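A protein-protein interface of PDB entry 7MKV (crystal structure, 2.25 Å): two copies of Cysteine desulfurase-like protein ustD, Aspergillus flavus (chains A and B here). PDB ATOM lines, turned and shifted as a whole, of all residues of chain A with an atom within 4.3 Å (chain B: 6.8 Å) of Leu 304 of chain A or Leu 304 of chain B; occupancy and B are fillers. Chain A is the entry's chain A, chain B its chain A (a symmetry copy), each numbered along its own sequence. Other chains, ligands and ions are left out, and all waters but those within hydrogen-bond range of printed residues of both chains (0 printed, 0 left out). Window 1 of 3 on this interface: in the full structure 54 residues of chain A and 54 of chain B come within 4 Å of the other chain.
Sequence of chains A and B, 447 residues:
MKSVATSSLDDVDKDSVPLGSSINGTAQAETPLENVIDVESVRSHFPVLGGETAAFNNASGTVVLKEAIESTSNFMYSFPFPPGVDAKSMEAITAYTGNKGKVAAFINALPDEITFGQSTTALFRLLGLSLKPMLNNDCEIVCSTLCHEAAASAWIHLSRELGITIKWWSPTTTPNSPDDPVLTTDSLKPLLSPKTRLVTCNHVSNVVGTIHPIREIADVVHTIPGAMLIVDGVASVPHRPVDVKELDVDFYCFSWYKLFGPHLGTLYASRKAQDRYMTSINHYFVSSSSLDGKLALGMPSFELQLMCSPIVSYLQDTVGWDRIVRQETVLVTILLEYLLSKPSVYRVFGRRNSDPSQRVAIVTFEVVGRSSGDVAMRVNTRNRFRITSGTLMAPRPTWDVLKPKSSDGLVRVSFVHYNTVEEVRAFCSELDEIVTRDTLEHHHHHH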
ATOM      1  N   PRO A 262      25.674  25.874 -15.706  1.00  0.00           N
ATOM      2  CA  PRO A 262      26.675  24.938 -15.194  1.00  0.00           C
ATOM      3  C   PRO A 262      28.118  25.364 -15.505  1.00  0.00           C
ATOM      4  O   PRO A 262      28.308  26.257 -16.317  1.00  0.00           O
ATOM      5  CB  PRO A 262      26.333  23.641 -15.942  1.00  0.00           C
ATOM      6  CG  PRO A 262      25.776  24.118 -17.269  1.00  0.00           C
ATOM      7  CD  PRO A 262      25.026  25.391 -16.936  1.00  0.00           C
ATOM      8  N   HIS A 263      29.093  24.730 -14.846  1.00  0.00           N
ATOM      9  CA  HIS A 263      30.537  24.819 -15.192  1.00  0.00           C
ATOM     10  C   HIS A 263      30.745  24.059 -16.506  1.00  0.00           C
ATOM     11  O   HIS A 263      30.912  22.828 -16.459  1.00  0.00           O
ATOM     12  CB  HIS A 263      31.416  24.303 -14.046  1.00  0.00           C
ATOM     13  CG  HIS A 263      31.389  25.167 -12.830  1.00  0.00           C
ATOM     14  ND1 HIS A 263      30.446  25.009 -11.834  1.00  0.00           N
ATOM     15  CD2 HIS A 263      32.179  26.191 -12.443  1.00  0.00           C
ATOM     16  CE1 HIS A 263      30.653  25.904 -10.888  1.00  0.00           C
ATOM     17  NE2 HIS A 263      31.715  26.638 -11.236  1.00  0.00           N
ATOM     18  N   LEU A 264      30.693  24.784 -17.626  1.00  0.00           N
ATOM     19  CA  LEU A 264      30.613  24.245 -19.009  1.00  0.00           C
ATOM     20  C   LEU A 264      30.968  25.371 -19.988  1.00  0.00           C
ATOM     21  O   LEU A 264      30.405  26.480 -19.850  1.00  0.00           O
ATOM     22  CB  LEU A 264      29.191  23.729 -19.254  1.00  0.00           C
ATOM     23  CG  LEU A 264      28.938  23.083 -20.618  1.00  0.00           C
ATOM     24  CD1 LEU A 264      29.439  21.645 -20.638  1.00  0.00           C
ATOM     25  CD2 LEU A 264      27.462  23.132 -20.979  1.00  0.00           C
ATOM     26  N   SER A 301      28.774  15.948 -22.201  1.00  0.00           N
ATOM     27  CA  SER A 301      27.921  16.055 -20.991  1.00  0.00           C
ATOM     28  C   SER A 301      26.558  16.622 -21.388  1.00  0.00           C
ATOM     29  O   SER A 301      26.348  17.836 -21.209  1.00  0.00           O
ATOM     30  CB  SER A 301      28.578  16.890 -19.926  1.00  0.00           C
ATOM     31  OG  SER A 301      27.742  16.976 -18.781  1.00  0.00           O
ATOM     32  N   PHE A 302      25.671  15.768 -21.906  1.00  0.00           N
ATOM     33  CA  PHE A 302      24.324  16.151 -22.407  1.00  0.00           C
ATOM     34  C   PHE A 302      23.527  16.811 -21.277  1.00  0.00           C
ATOM     35  O   PHE A 302      22.796  17.778 -21.555  1.00  0.00           O
ATOM     36  CB  PHE A 302      23.557  14.942 -22.944  1.00  0.00           C
ATOM     37  CG  PHE A 302      24.304  14.110 -23.957  1.00  0.00           C
ATOM     38  CD1 PHE A 302      24.455  14.545 -25.265  1.00  0.00           C
ATOM     39  CD2 PHE A 302      24.843  12.883 -23.602  1.00  0.00           C
ATOM     40  CE1 PHE A 302      25.137  13.773 -26.193  1.00  0.00           C
ATOM     41  CE2 PHE A 302      25.523  12.112 -24.532  1.00  0.00           C
ATOM     42  CZ  PHE A 302      25.670  12.559 -25.825  1.00  0.00           C
ATOM     43  N   GLU A 303      23.663  16.291 -20.050  1.00  0.00           N
ATOM     44  CA  GLU A 303      22.911  16.758 -18.852  1.00  0.00           C
ATOM     45  C   GLU A 303      23.232  18.235 -18.572  1.00  0.00           C
ATOM     46  O   GLU A 303      22.305  18.961 -18.171  1.00  0.00           O
ATOM     47  CB  GLU A 303      23.175  15.862 -17.635  1.00  0.00           C
ATOM     48  CG  GLU A 303      24.628  15.783 -17.190  1.00  0.00           C
ATOM     49  CD  GLU A 303      25.445  14.658 -17.803  1.00  0.00           C
ATOM     50  OE1 GLU A 303      24.958  14.012 -18.754  1.00  0.00           O
ATOM     51  OE2 GLU A 303      26.576  14.434 -17.331  1.00  0.00           O
ATOM     52  N   LEU A 304      24.475  18.675 -18.801  1.00  0.00           N
ATOM     53  CA  LEU A 304      24.905  20.081 -18.561  1.00  0.00           C
ATOM     54  C   LEU A 304      24.481  20.965 -19.742  1.00  0.00           C
ATOM     55  O   LEU A 304      24.059  22.107 -19.495  1.00  0.00           O
ATOM     56  CB  LEU A 304      26.421  20.133 -18.341  1.00  0.00           C
ATOM     57  CG  LEU A 304      26.933  19.535 -17.030  1.00  0.00           C
ATOM     58  CD1 LEU A 304      28.401  19.880 -16.825  1.00  0.00           C
ATOM     59  CD2 LEU A 304      26.111  20.004 -15.837  1.00  0.00           C
ATOM     60  N   GLN A 305      24.582  20.460 -20.976  1.00  0.00           N
ATOM     61  CA  GLN A 305      24.198  21.209 -22.204  1.00  0.00           C
ATOM     62  C   GLN A 305      22.723  21.620 -22.118  1.00  0.00           C
ATOM     63  O   GLN A 305      22.416  22.780 -22.444  1.00  0.00           O
ATOM     64  CB  GLN A 305      24.408  20.372 -23.465  1.00  0.00           C
ATOM     65  CG  GLN A 305      25.866  20.063 -23.771  1.00  0.00           C
ATOM     66  CD  GLN A 305      26.015  19.257 -25.039  1.00  0.00           C
ATOM     67  OE1 GLN A 305      25.080  19.129 -25.832  1.00  0.00           O
ATOM     68  NE2 GLN A 305      27.203  18.708 -25.244  1.00  0.00           N
ATOM     69  N   LEU A 306      21.855  20.699 -21.692  1.00  0.00           N
ATOM     70  CA  LEU A 306      20.377  20.879 -21.681  1.00  0.00           C
ATOM     71  C   LEU A 306      19.953  21.842 -20.560  1.00  0.00           C
ATOM     72  O   LEU A 306      18.754  22.164 -20.503  1.00  0.00           O
ATOM     73  CB  LEU A 306      19.705  19.507 -21.553  1.00  0.00           C
ATOM     74  CG  LEU A 306      19.537  18.760 -22.876  1.00  0.00           C
ATOM     75  CD1 LEU A 306      19.434  17.263 -22.657  1.00  0.00           C
ATOM     76  CD2 LEU A 306      18.321  19.266 -23.634  1.00  0.00           C
ATOM     77  N   MET A 307      20.892  22.303 -19.724  1.00  0.00           N
ATOM     78  CA  MET A 307      20.672  23.407 -18.747  1.00  0.00           C
ATOM     79  C   MET A 307      20.699  24.773 -19.455  1.00  0.00           C
ATOM     80  O   MET A 307      20.300  25.766 -18.816  1.00  0.00           O
ATOM     81  CB  MET A 307      21.751  23.412 -17.661  1.00  0.00           C
ATOM     82  CG  MET A 307      21.704  22.209 -16.754  1.00  0.00           C
ATOM     83  SD  MET A 307      22.900  22.286 -15.397  1.00  0.00           S
ATOM     84  CE  MET A 307      22.266  23.673 -14.458  1.00  0.00           C
ATOM     85  N   CYS A 308      21.155  24.838 -20.711  1.00  0.00           N
ATOM     86  CA  CYS A 308      21.581  26.105 -21.370  1.00  0.00           C
ATOM     87  C   CYS A 308      20.418  26.795 -22.098  1.00  0.00           C
ATOM     88  O   CYS A 308      20.354  28.041 -22.019  1.00  0.00           O
ATOM     89  CB  CYS A 308      22.757  25.864 -22.305  1.00  0.00           C
ATOM     90  SG  CYS A 308      24.248  25.356 -21.410  1.00  0.00           S
ATOM     91  N   ALA B  68      22.159  10.536  -6.719  1.00  0.00           N
ATOM     92  CA  ALA B  68      23.163  11.351  -7.447  1.00  0.00           C
ATOM     93  C   ALA B  68      22.505  12.630  -7.982  1.00  0.00           C
ATOM     94  O   ALA B  68      23.114  13.705  -7.838  1.00  0.00           O
ATOM     95  CB  ALA B  68      23.790  10.541  -8.558  1.00  0.00           C
ATOM     96  N   THR B  72      23.200  16.747  -6.750  1.00  0.00           N
ATOM     97  CA  THR B  72      23.617  17.832  -7.685  1.00  0.00           C
ATOM     98  C   THR B  72      22.573  18.957  -7.659  1.00  0.00           C
ATOM     99  O   THR B  72      22.988  20.131  -7.689  1.00  0.00           O
ATOM    100  CB  THR B  72      23.902  17.292  -9.094  1.00  0.00           C
ATOM    101  OG1 THR B  72      24.612  18.300  -9.816  1.00  0.00           O
ATOM    102  CG2 THR B  72      22.666  16.900  -9.874  1.00  0.00           C
ATOM    103  N   PHE B  75      23.220  21.022  -4.493  1.00  0.00           N
ATOM    104  CA  PHE B  75      24.444  21.839  -4.700  1.00  0.00           C
ATOM    105  C   PHE B  75      24.120  23.047  -5.592  1.00  0.00           C
ATOM    106  O   PHE B  75      24.538  24.171  -5.252  1.00  0.00           O
ATOM    107  CB  PHE B  75      25.577  21.010  -5.309  1.00  0.00           C
ATOM    108  CG  PHE B  75      26.800  21.826  -5.640  1.00  0.00           C
ATOM    109  CD1 PHE B  75      27.726  22.146  -4.656  1.00  0.00           C
ATOM    110  CD2 PHE B  75      27.008  22.310  -6.925  1.00  0.00           C
ATOM    111  CE1 PHE B  75      28.843  22.911  -4.957  1.00  0.00           C
ATOM    112  CE2 PHE B  75      28.125  23.075  -7.222  1.00  0.00           C
ATOM    113  CZ  PHE B  75      29.038  23.375  -6.237  1.00  0.00           C
ATOM    114  N   MET B  76      23.403  22.822  -6.697  1.00  0.00           N
ATOM    115  CA  MET B  76      23.135  23.858  -7.732  1.00  0.00           C
ATOM    116  C   MET B  76      22.081  24.860  -7.228  1.00  0.00           C
ATOM    117  O   MET B  76      22.084  25.994  -7.730  1.00  0.00           O
ATOM    118  CB  MET B  76      22.690  23.214  -9.051  1.00  0.00           C
ATOM    119  CG  MET B  76      23.836  22.534  -9.787  1.00  0.00           C
ATOM    120  SD  MET B  76      23.415  21.948 -11.453  1.00  0.00           S
ATOM    121  CE  MET B  76      22.252  20.641 -11.070  1.00  0.00           C
ATOM    122  N   ASN B  99      33.494  14.511  -0.556  1.00  0.00           N
ATOM    123  CA  ASN B  99      33.061  13.841  -1.813  1.00  0.00           C
ATOM    124  C   ASN B  99      34.287  13.279  -2.540  1.00  0.00           C
ATOM    125  O   ASN B  99      34.226  12.113  -2.978  1.00  0.00           O
ATOM    126  CB  ASN B  99      32.278  14.789  -2.725  1.00  0.00           C
ATOM    127  CG  ASN B  99      31.972  14.190  -4.083  1.00  0.00           C
ATOM    128  OD1 ASN B  99      31.027  13.419  -4.225  1.00  0.00           O
ATOM    129  ND2 ASN B  99      32.759  14.545  -5.087  1.00  0.00           N
ATOM    130  N   PHE B 116      39.138  14.870 -11.497  1.00  0.00           N
ATOM    131  CA  PHE B 116      37.925  14.788 -12.350  1.00  0.00           C
ATOM    132  C   PHE B 116      38.194  15.553 -13.648  1.00  0.00           C
ATOM    133  O   PHE B 116      38.863  16.598 -13.593  1.00  0.00           O
ATOM    134  CB  PHE B 116      36.705  15.349 -11.620  1.00  0.00           C
ATOM    135  CG  PHE B 116      36.292  14.581 -10.390  1.00  0.00           C
ATOM    136  CD1 PHE B 116      35.399  13.525 -10.482  1.00  0.00           C
ATOM    137  CD2 PHE B 116      36.769  14.938  -9.137  1.00  0.00           C
ATOM    138  CE1 PHE B 116      35.004  12.833  -9.347  1.00  0.00           C
ATOM    139  CE2 PHE B 116      36.369  14.247  -8.002  1.00  0.00           C
ATOM    140  CZ  PHE B 116      35.488  13.196  -8.110  1.00  0.00           C
ATOM    141  N   GLY B 117      37.697  15.033 -14.773  1.00  0.00           N
ATOM    142  CA  GLY B 117      37.845  15.644 -16.107  1.00  0.00           C
ATOM    143  C   GLY B 117      36.573  15.515 -16.923  1.00  0.00           C
ATOM    144  O   GLY B 117      35.610  14.908 -16.427  1.00  0.00           O
ATOM    145  N   GLN B 118      36.584  16.062 -18.138  1.00  0.00           N
ATOM    146  CA  GLN B 118      35.443  16.070 -19.091  1.00  0.00           C
ATOM    147  C   GLN B 118      35.026  14.633 -19.420  1.00  0.00           C
ATOM    148  O   GLN B 118      33.816  14.365 -19.451  1.00  0.00           O
ATOM    149  CB  GLN B 118      35.866  16.814 -20.355  1.00  0.00           C
ATOM    150  CG  GLN B 118      34.812  16.868 -21.452  1.00  0.00           C
ATOM    151  CD  GLN B 118      35.421  17.361 -22.742  1.00  0.00           C
ATOM    152  OE1 GLN B 118      36.340  18.180 -22.742  1.00  0.00           O
ATOM    153  NE2 GLN B 118      34.932  16.842 -23.857  1.00  0.00           N
ATOM    154  N   TRP B 256      32.027   7.958 -15.372  1.00  0.00           N
ATOM    155  CA  TRP B 256      30.941   7.773 -14.374  1.00  0.00           C
ATOM    156  C   TRP B 256      29.608   7.412 -15.046  1.00  0.00           C
ATOM    157  O   TRP B 256      28.769   6.794 -14.362  1.00  0.00           O
ATOM    158  CB  TRP B 256      30.823   9.010 -13.478  1.00  0.00           C
ATOM    159  CG  TRP B 256      31.888   9.069 -12.429  1.00  0.00           C
ATOM    160  CD1 TRP B 256      33.055   9.776 -12.473  1.00  0.00           C
ATOM    161  CD2 TRP B 256      31.891   8.367 -11.174  1.00  0.00           C
ATOM    162  NE1 TRP B 256      33.776   9.570 -11.329  1.00  0.00           N
ATOM    163  CE2 TRP B 256      33.087   8.715 -10.511  1.00  0.00           C
ATOM    164  CE3 TRP B 256      31.001   7.491 -10.545  1.00  0.00           C
ATOM    165  CZ2 TRP B 256      33.415   8.212  -9.253  1.00  0.00           C
ATOM    166  CZ3 TRP B 256      31.326   6.992  -9.301  1.00  0.00           C
ATOM    167  CH2 TRP B 256      32.517   7.350  -8.666  1.00  0.00           C
ATOM    168  N   GLY B 261      26.105   7.349 -13.125  1.00  0.00           N
ATOM    169  CA  GLY B 261      26.543   8.717 -12.791  1.00  0.00           C
ATOM    170  C   GLY B 261      26.512   9.658 -13.994  1.00  0.00           C
ATOM    171  O   GLY B 261      25.925   9.349 -15.031  1.00  0.00           O
ATOM    172  N   PRO B 262      27.137  10.851 -13.872  1.00  0.00           N
ATOM    173  CA  PRO B 262      27.192  11.819 -14.968  1.00  0.00           C
ATOM    174  C   PRO B 262      28.240  11.467 -16.035  1.00  0.00           C
ATOM    175  O   PRO B 262      29.069  10.604 -15.786  1.00  0.00           O
ATOM    176  CB  PRO B 262      27.585  13.117 -14.248  1.00  0.00           C
ATOM    177  CG  PRO B 262      28.434  12.648 -13.083  1.00  0.00           C
ATOM    178  CD  PRO B 262      27.812  11.335 -12.657  1.00  0.00           C
ATOM    179  N   HIS B 263      28.170  12.128 -17.194  1.00  0.00           N
ATOM    180  CA  HIS B 263      29.233  12.114 -18.235  1.00  0.00           C
ATOM    181  C   HIS B 263      30.421  12.916 -17.693  1.00  0.00           C
ATOM    182  O   HIS B 263      30.413  14.151 -17.829  1.00  0.00           O
ATOM    183  CB  HIS B 263      28.705  12.640 -19.576  1.00  0.00           C
ATOM    184  CG  HIS B 263      27.700  11.745 -20.221  1.00  0.00           C
ATOM    185  ND1 HIS B 263      26.350  11.835 -19.948  1.00  0.00           N
ATOM    186  CD2 HIS B 263      27.839  10.750 -21.122  1.00  0.00           C
ATOM    187  CE1 HIS B 263      25.700  10.927 -20.650  1.00  0.00           C
ATOM    188  NE2 HIS B 263      26.591  10.251 -21.382  1.00  0.00           N
ATOM    189  N   LEU B 264      31.374  12.217 -17.072  1.00  0.00           N
ATOM    190  CA  LEU B 264      32.478  12.787 -16.256  1.00  0.00           C
ATOM    191  C   LEU B 264      33.546  11.703 -16.064  1.00  0.00           C
ATOM    192  O   LEU B 264      33.182  10.567 -15.689  1.00  0.00           O
ATOM    193  CB  LEU B 264      31.908  13.243 -14.908  1.00  0.00           C
ATOM    194  CG  LEU B 264      32.898  13.911 -13.953  1.00  0.00           C
ATOM    195  CD1 LEU B 264      33.116  15.371 -14.330  1.00  0.00           C
ATOM    196  CD2 LEU B 264      32.424  13.805 -12.512  1.00  0.00           C
ATOM    197  N   SER B 301      33.826  21.069 -12.792  1.00  0.00           N
ATOM    198  CA  SER B 301      32.354  20.893 -12.716  1.00  0.00           C
ATOM    199  C   SER B 301      31.993  20.274 -11.365  1.00  0.00           C
ATOM    200  O   SER B 301      31.786  19.048 -11.313  1.00  0.00           O
ATOM    201  CB  SER B 301      31.839  20.062 -13.859  1.00  0.00           C
ATOM    202  OG  SER B 301      30.431  19.909 -13.763  1.00  0.00           O
ATOM    203  N   PHE B 302      31.923  21.100 -10.317  1.00  0.00           N
ATOM    204  CA  PHE B 302      31.650  20.668  -8.921  1.00  0.00           C
ATOM    205  C   PHE B 302      30.300  19.945  -8.863  1.00  0.00           C
ATOM    206  O   PHE B 302      30.193  18.953  -8.121  1.00  0.00           O
ATOM    207  CB  PHE B 302      31.643  21.855  -7.955  1.00  0.00           C
ATOM    208  CG  PHE B 302      32.858  22.745  -8.028  1.00  0.00           C
ATOM    209  CD1 PHE B 302      34.065  22.350  -7.472  1.00  0.00           C
ATOM    210  CD2 PHE B 302      32.788  23.985  -8.641  1.00  0.00           C
ATOM    211  CE1 PHE B 302      35.178  23.176  -7.536  1.00  0.00           C
ATOM    212  CE2 PHE B 302      33.900  24.810  -8.704  1.00  0.00           C
ATOM    213  CZ  PHE B 302      35.094  24.403  -8.152  1.00  0.00           C
ATOM    214  N   GLU B 303      29.310  20.439  -9.618  1.00  0.00           N
ATOM    215  CA  GLU B 303      27.919  19.908  -9.630  1.00  0.00           C
ATOM    216  C   GLU B 303      27.920  18.440 -10.088  1.00  0.00           C
ATOM    217  O   GLU B 303      27.122  17.663  -9.534  1.00  0.00           O
ATOM    218  CB  GLU B 303      26.988  20.784 -10.478  1.00  0.00           C
ATOM    219  CG  GLU B 303      27.378  20.918 -11.942  1.00  0.00           C
ATOM    220  CD  GLU B 303      28.278  22.095 -12.280  1.00  0.00           C
ATOM    221  OE1 GLU B 303      28.796  22.741 -11.345  1.00  0.00           O
ATOM    222  OE2 GLU B 303      28.469  22.358 -13.482  1.00  0.00           O
ATOM    223  N   LEU B 304      28.792  18.064 -11.030  1.00  0.00           N
ATOM    224  CA  LEU B 304      28.882  16.673 -11.556  1.00  0.00           C
ATOM    225  C   LEU B 304      29.697  15.801 -10.592  1.00  0.00           C
ATOM    226  O   LEU B 304      29.316  14.635 -10.395  1.00  0.00           O
ATOM    227  CB  LEU B 304      29.502  16.685 -12.958  1.00  0.00           C
ATOM    228  CG  LEU B 304      28.636  17.273 -14.074  1.00  0.00           C
ATOM    229  CD1 LEU B 304      29.257  16.990 -15.434  1.00  0.00           C
ATOM    230  CD2 LEU B 304      27.212  16.736 -14.024  1.00  0.00           C
ATOM    231  N   GLN B 305      30.772  16.341 -10.009  1.00  0.00           N
ATOM    232  CA  GLN B 305      31.642  15.606  -9.050  1.00  0.00           C
ATOM    233  C   GLN B 305      30.806  15.126  -7.857  1.00  0.00           C
ATOM    234  O   GLN B 305      30.972  13.962  -7.453  1.00  0.00           O
ATOM    235  CB  GLN B 305      32.783  16.484  -8.535  1.00  0.00           C
ATOM    236  CG  GLN B 305      33.801  16.866  -9.599  1.00  0.00           C
ATOM    237  CD  GLN B 305      34.917  17.711  -9.031  1.00  0.00           C
ATOM    238  OE1 GLN B 305      35.087  17.816  -7.815  1.00  0.00           O
ATOM    239  NE2 GLN B 305      35.695  18.318  -9.914  1.00  0.00           N
ATOM    240  N   LEU B 306      29.942  15.995  -7.326  1.00  0.00           N
ATOM    241  CA  LEU B 306      29.158  15.749  -6.085  1.00  0.00           C
ATOM    242  C   LEU B 306      28.028  14.739  -6.346  1.00  0.00           C
ATOM    243  O   LEU B 306      27.358  14.361  -5.369  1.00  0.00           O
ATOM    244  CB  LEU B 306      28.630  17.085  -5.549  1.00  0.00           C
ATOM    245  CG  LEU B 306      29.628  17.856  -4.684  1.00  0.00           C
ATOM    246  CD1 LEU B 306      29.319  19.341  -4.676  1.00  0.00           C
ATOM    247  CD2 LEU B 306      29.647  17.314  -3.265  1.00  0.00           C
ATOM    248  N   MET B 307      27.839  14.300  -7.597  1.00  0.00           N
ATOM    249  CA  MET B 307      26.946  13.163  -7.958  1.00  0.00           C
ATOM    250  C   MET B 307      27.622  11.818  -7.639  1.00  0.00           C
ATOM    251  O   MET B 307      26.914  10.792  -7.666  1.00  0.00           O
ATOM    252  CB  MET B 307      26.600  13.180  -9.449  1.00  0.00           C
ATOM    253  CG  MET B 307      25.752  14.356  -9.861  1.00  0.00           C
ATOM    254  SD  MET B 307      25.241  14.300 -11.597  1.00  0.00           S
ATOM    255  CE  MET B 307      24.172  12.861 -11.595  1.00  0.00           C
ATOM    256  N   CYS B 308      28.930  11.806  -7.358  1.00  0.00           N
ATOM    257  CA  CYS B 308      29.772  10.576  -7.401  1.00  0.00           C
ATOM    258  C   CYS B 308      29.803   9.853  -6.047  1.00  0.00           C
ATOM    259  O   CYS B 308      29.759   8.604  -6.066  1.00  0.00           O
ATOM    260  CB  CYS B 308      31.176  10.895  -7.893  1.00  0.00           C
ATOM    261  SG  CYS B 308      31.186  11.447  -9.619  1.00  0.00           S
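The backbone NH (N) of His 263 of chain A lies within hydrogen-bond range of the side-chain carboxylate (OE2) of Glu 303 of chain B (2.8 Å).
N of His 263 of chain B is in hydrogen-bond range of OE2 of Glu 303 of chain A, at 2.8 Å.
The side-chain carboxylate (OE2) of Glu 303 of chain A is in hydrogen-bond range of the side-chain hydroxyl (OG) of Ser 301 of chain A, at 3.2 Å.
The backbone carbonyl oxygen (O) of Leu 304 of chain A is in hydrogen-bond range of the side-chain sulfur (SG) of Cys 308 of chain A (3.8 Å).
The backbone carbonyl oxygen (O) of Glu 303 of chain B is in hydrogen-bond range of the side-chain hydroxyl (OG1) of Thr 72 of chain B, at 2.6 Å.
The side-chain hydroxyl of Ser 301 of chain B lies within hydrogen-bond range of the side-chain carboxylate of Glu 303 of chain B, at 3.2 Å.
The backbone carbonyl oxygen (O) of Leu 304 of chain B is in hydrogen-bond range of the side-chain sulfur (SG) of Cys 308 of chain B (3.8 Å).
Among the printed residues, pairs that only touch across the chains: Leu 304 of chain A with Leu 304 of chain B (3.3 Å), Glu 303 of chain A with Pro 262 of chain B (3.5 Å), Pro 262 of chain A with Glu 303 of chain B (3.5 Å), Phe 302 of chain A with His 263 of chain B (3.6 Å), His 263 of chain A with Phe 302 of chain B (3.6 Å), Met 307 of chain A with Met 76 of chain B (3.7 Å), Leu 304 of chain A with Ser 301 of chain B (3.7 Å), Ser 301 of chain A with Leu 304 of chain B (3.7 Å), His 263 of chain A with Ser 301 of chain B (3.8 Å) and Ser 301 of chain A with His 263 of chain B (3.8 Å).
Leu 304 of chain A touches two residues of chain B.
Of chain A, only Ser 301 (3.7 Å) and Leu 304 (3.3 Å) come within 4 Å of Leu 304 of chain B.
Of the printed residues of chain A, Met 76 of chain B touches Met 307.
Of the printed residues of chain B, Glu 303 of chain A touches Pro 262 and His 263.
Leu 264 of chain A touches none of the printed residues of chain B.
Asn 99 of chain B touches none of the printed residues of chain A.
The nearest residue of chain B that does not touch Leu 304 of chain A is Glu 303 of chain B (4.1 Å).
Hydrophobic or aromatic side chains of chain A within 4 Å of the printed part of chain B: Pro 262, His 263, Phe 302, Leu 304 and Met 307.
Hydrophobic or aromatic side chains of chain B within 4 Å of the printed part of chain A: Met 76, Pro 262, His 263, Phe 302 and Leu 304.
Along chain B the printed residues that touch a printed residue of chain A span positions 76 to 304.
Among the printed residues, 12 pairs touch across the chains.
Among the printed residues, no Asp or Glu carboxylate lies within 4 Å of a Lys or Arg side-chain nitrogen of the other chain.
Pro 262 of chain A touches Glu 303 of chain B, and with the chains exchanged Glu 303 of chain A touches Pro 262 of chain B.
His 263 of chain A touches Ser 301 of chain B, and with the chains exchanged Ser 301 of chain A touches His 263 of chain B.
His 263 of chain A touches Phe 302 of chain B, and with the chains exchanged Phe 302 of chain A touches His 263 of chain B.
His 263 of chain A touches Glu 303 of chain B, and with the chains exchanged Glu 303 of chain A touches His 263 of chain B.
Of the 12 pairs that touch across the chains among the printed residues, 11 have their exchanged pair printed and touching as well.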
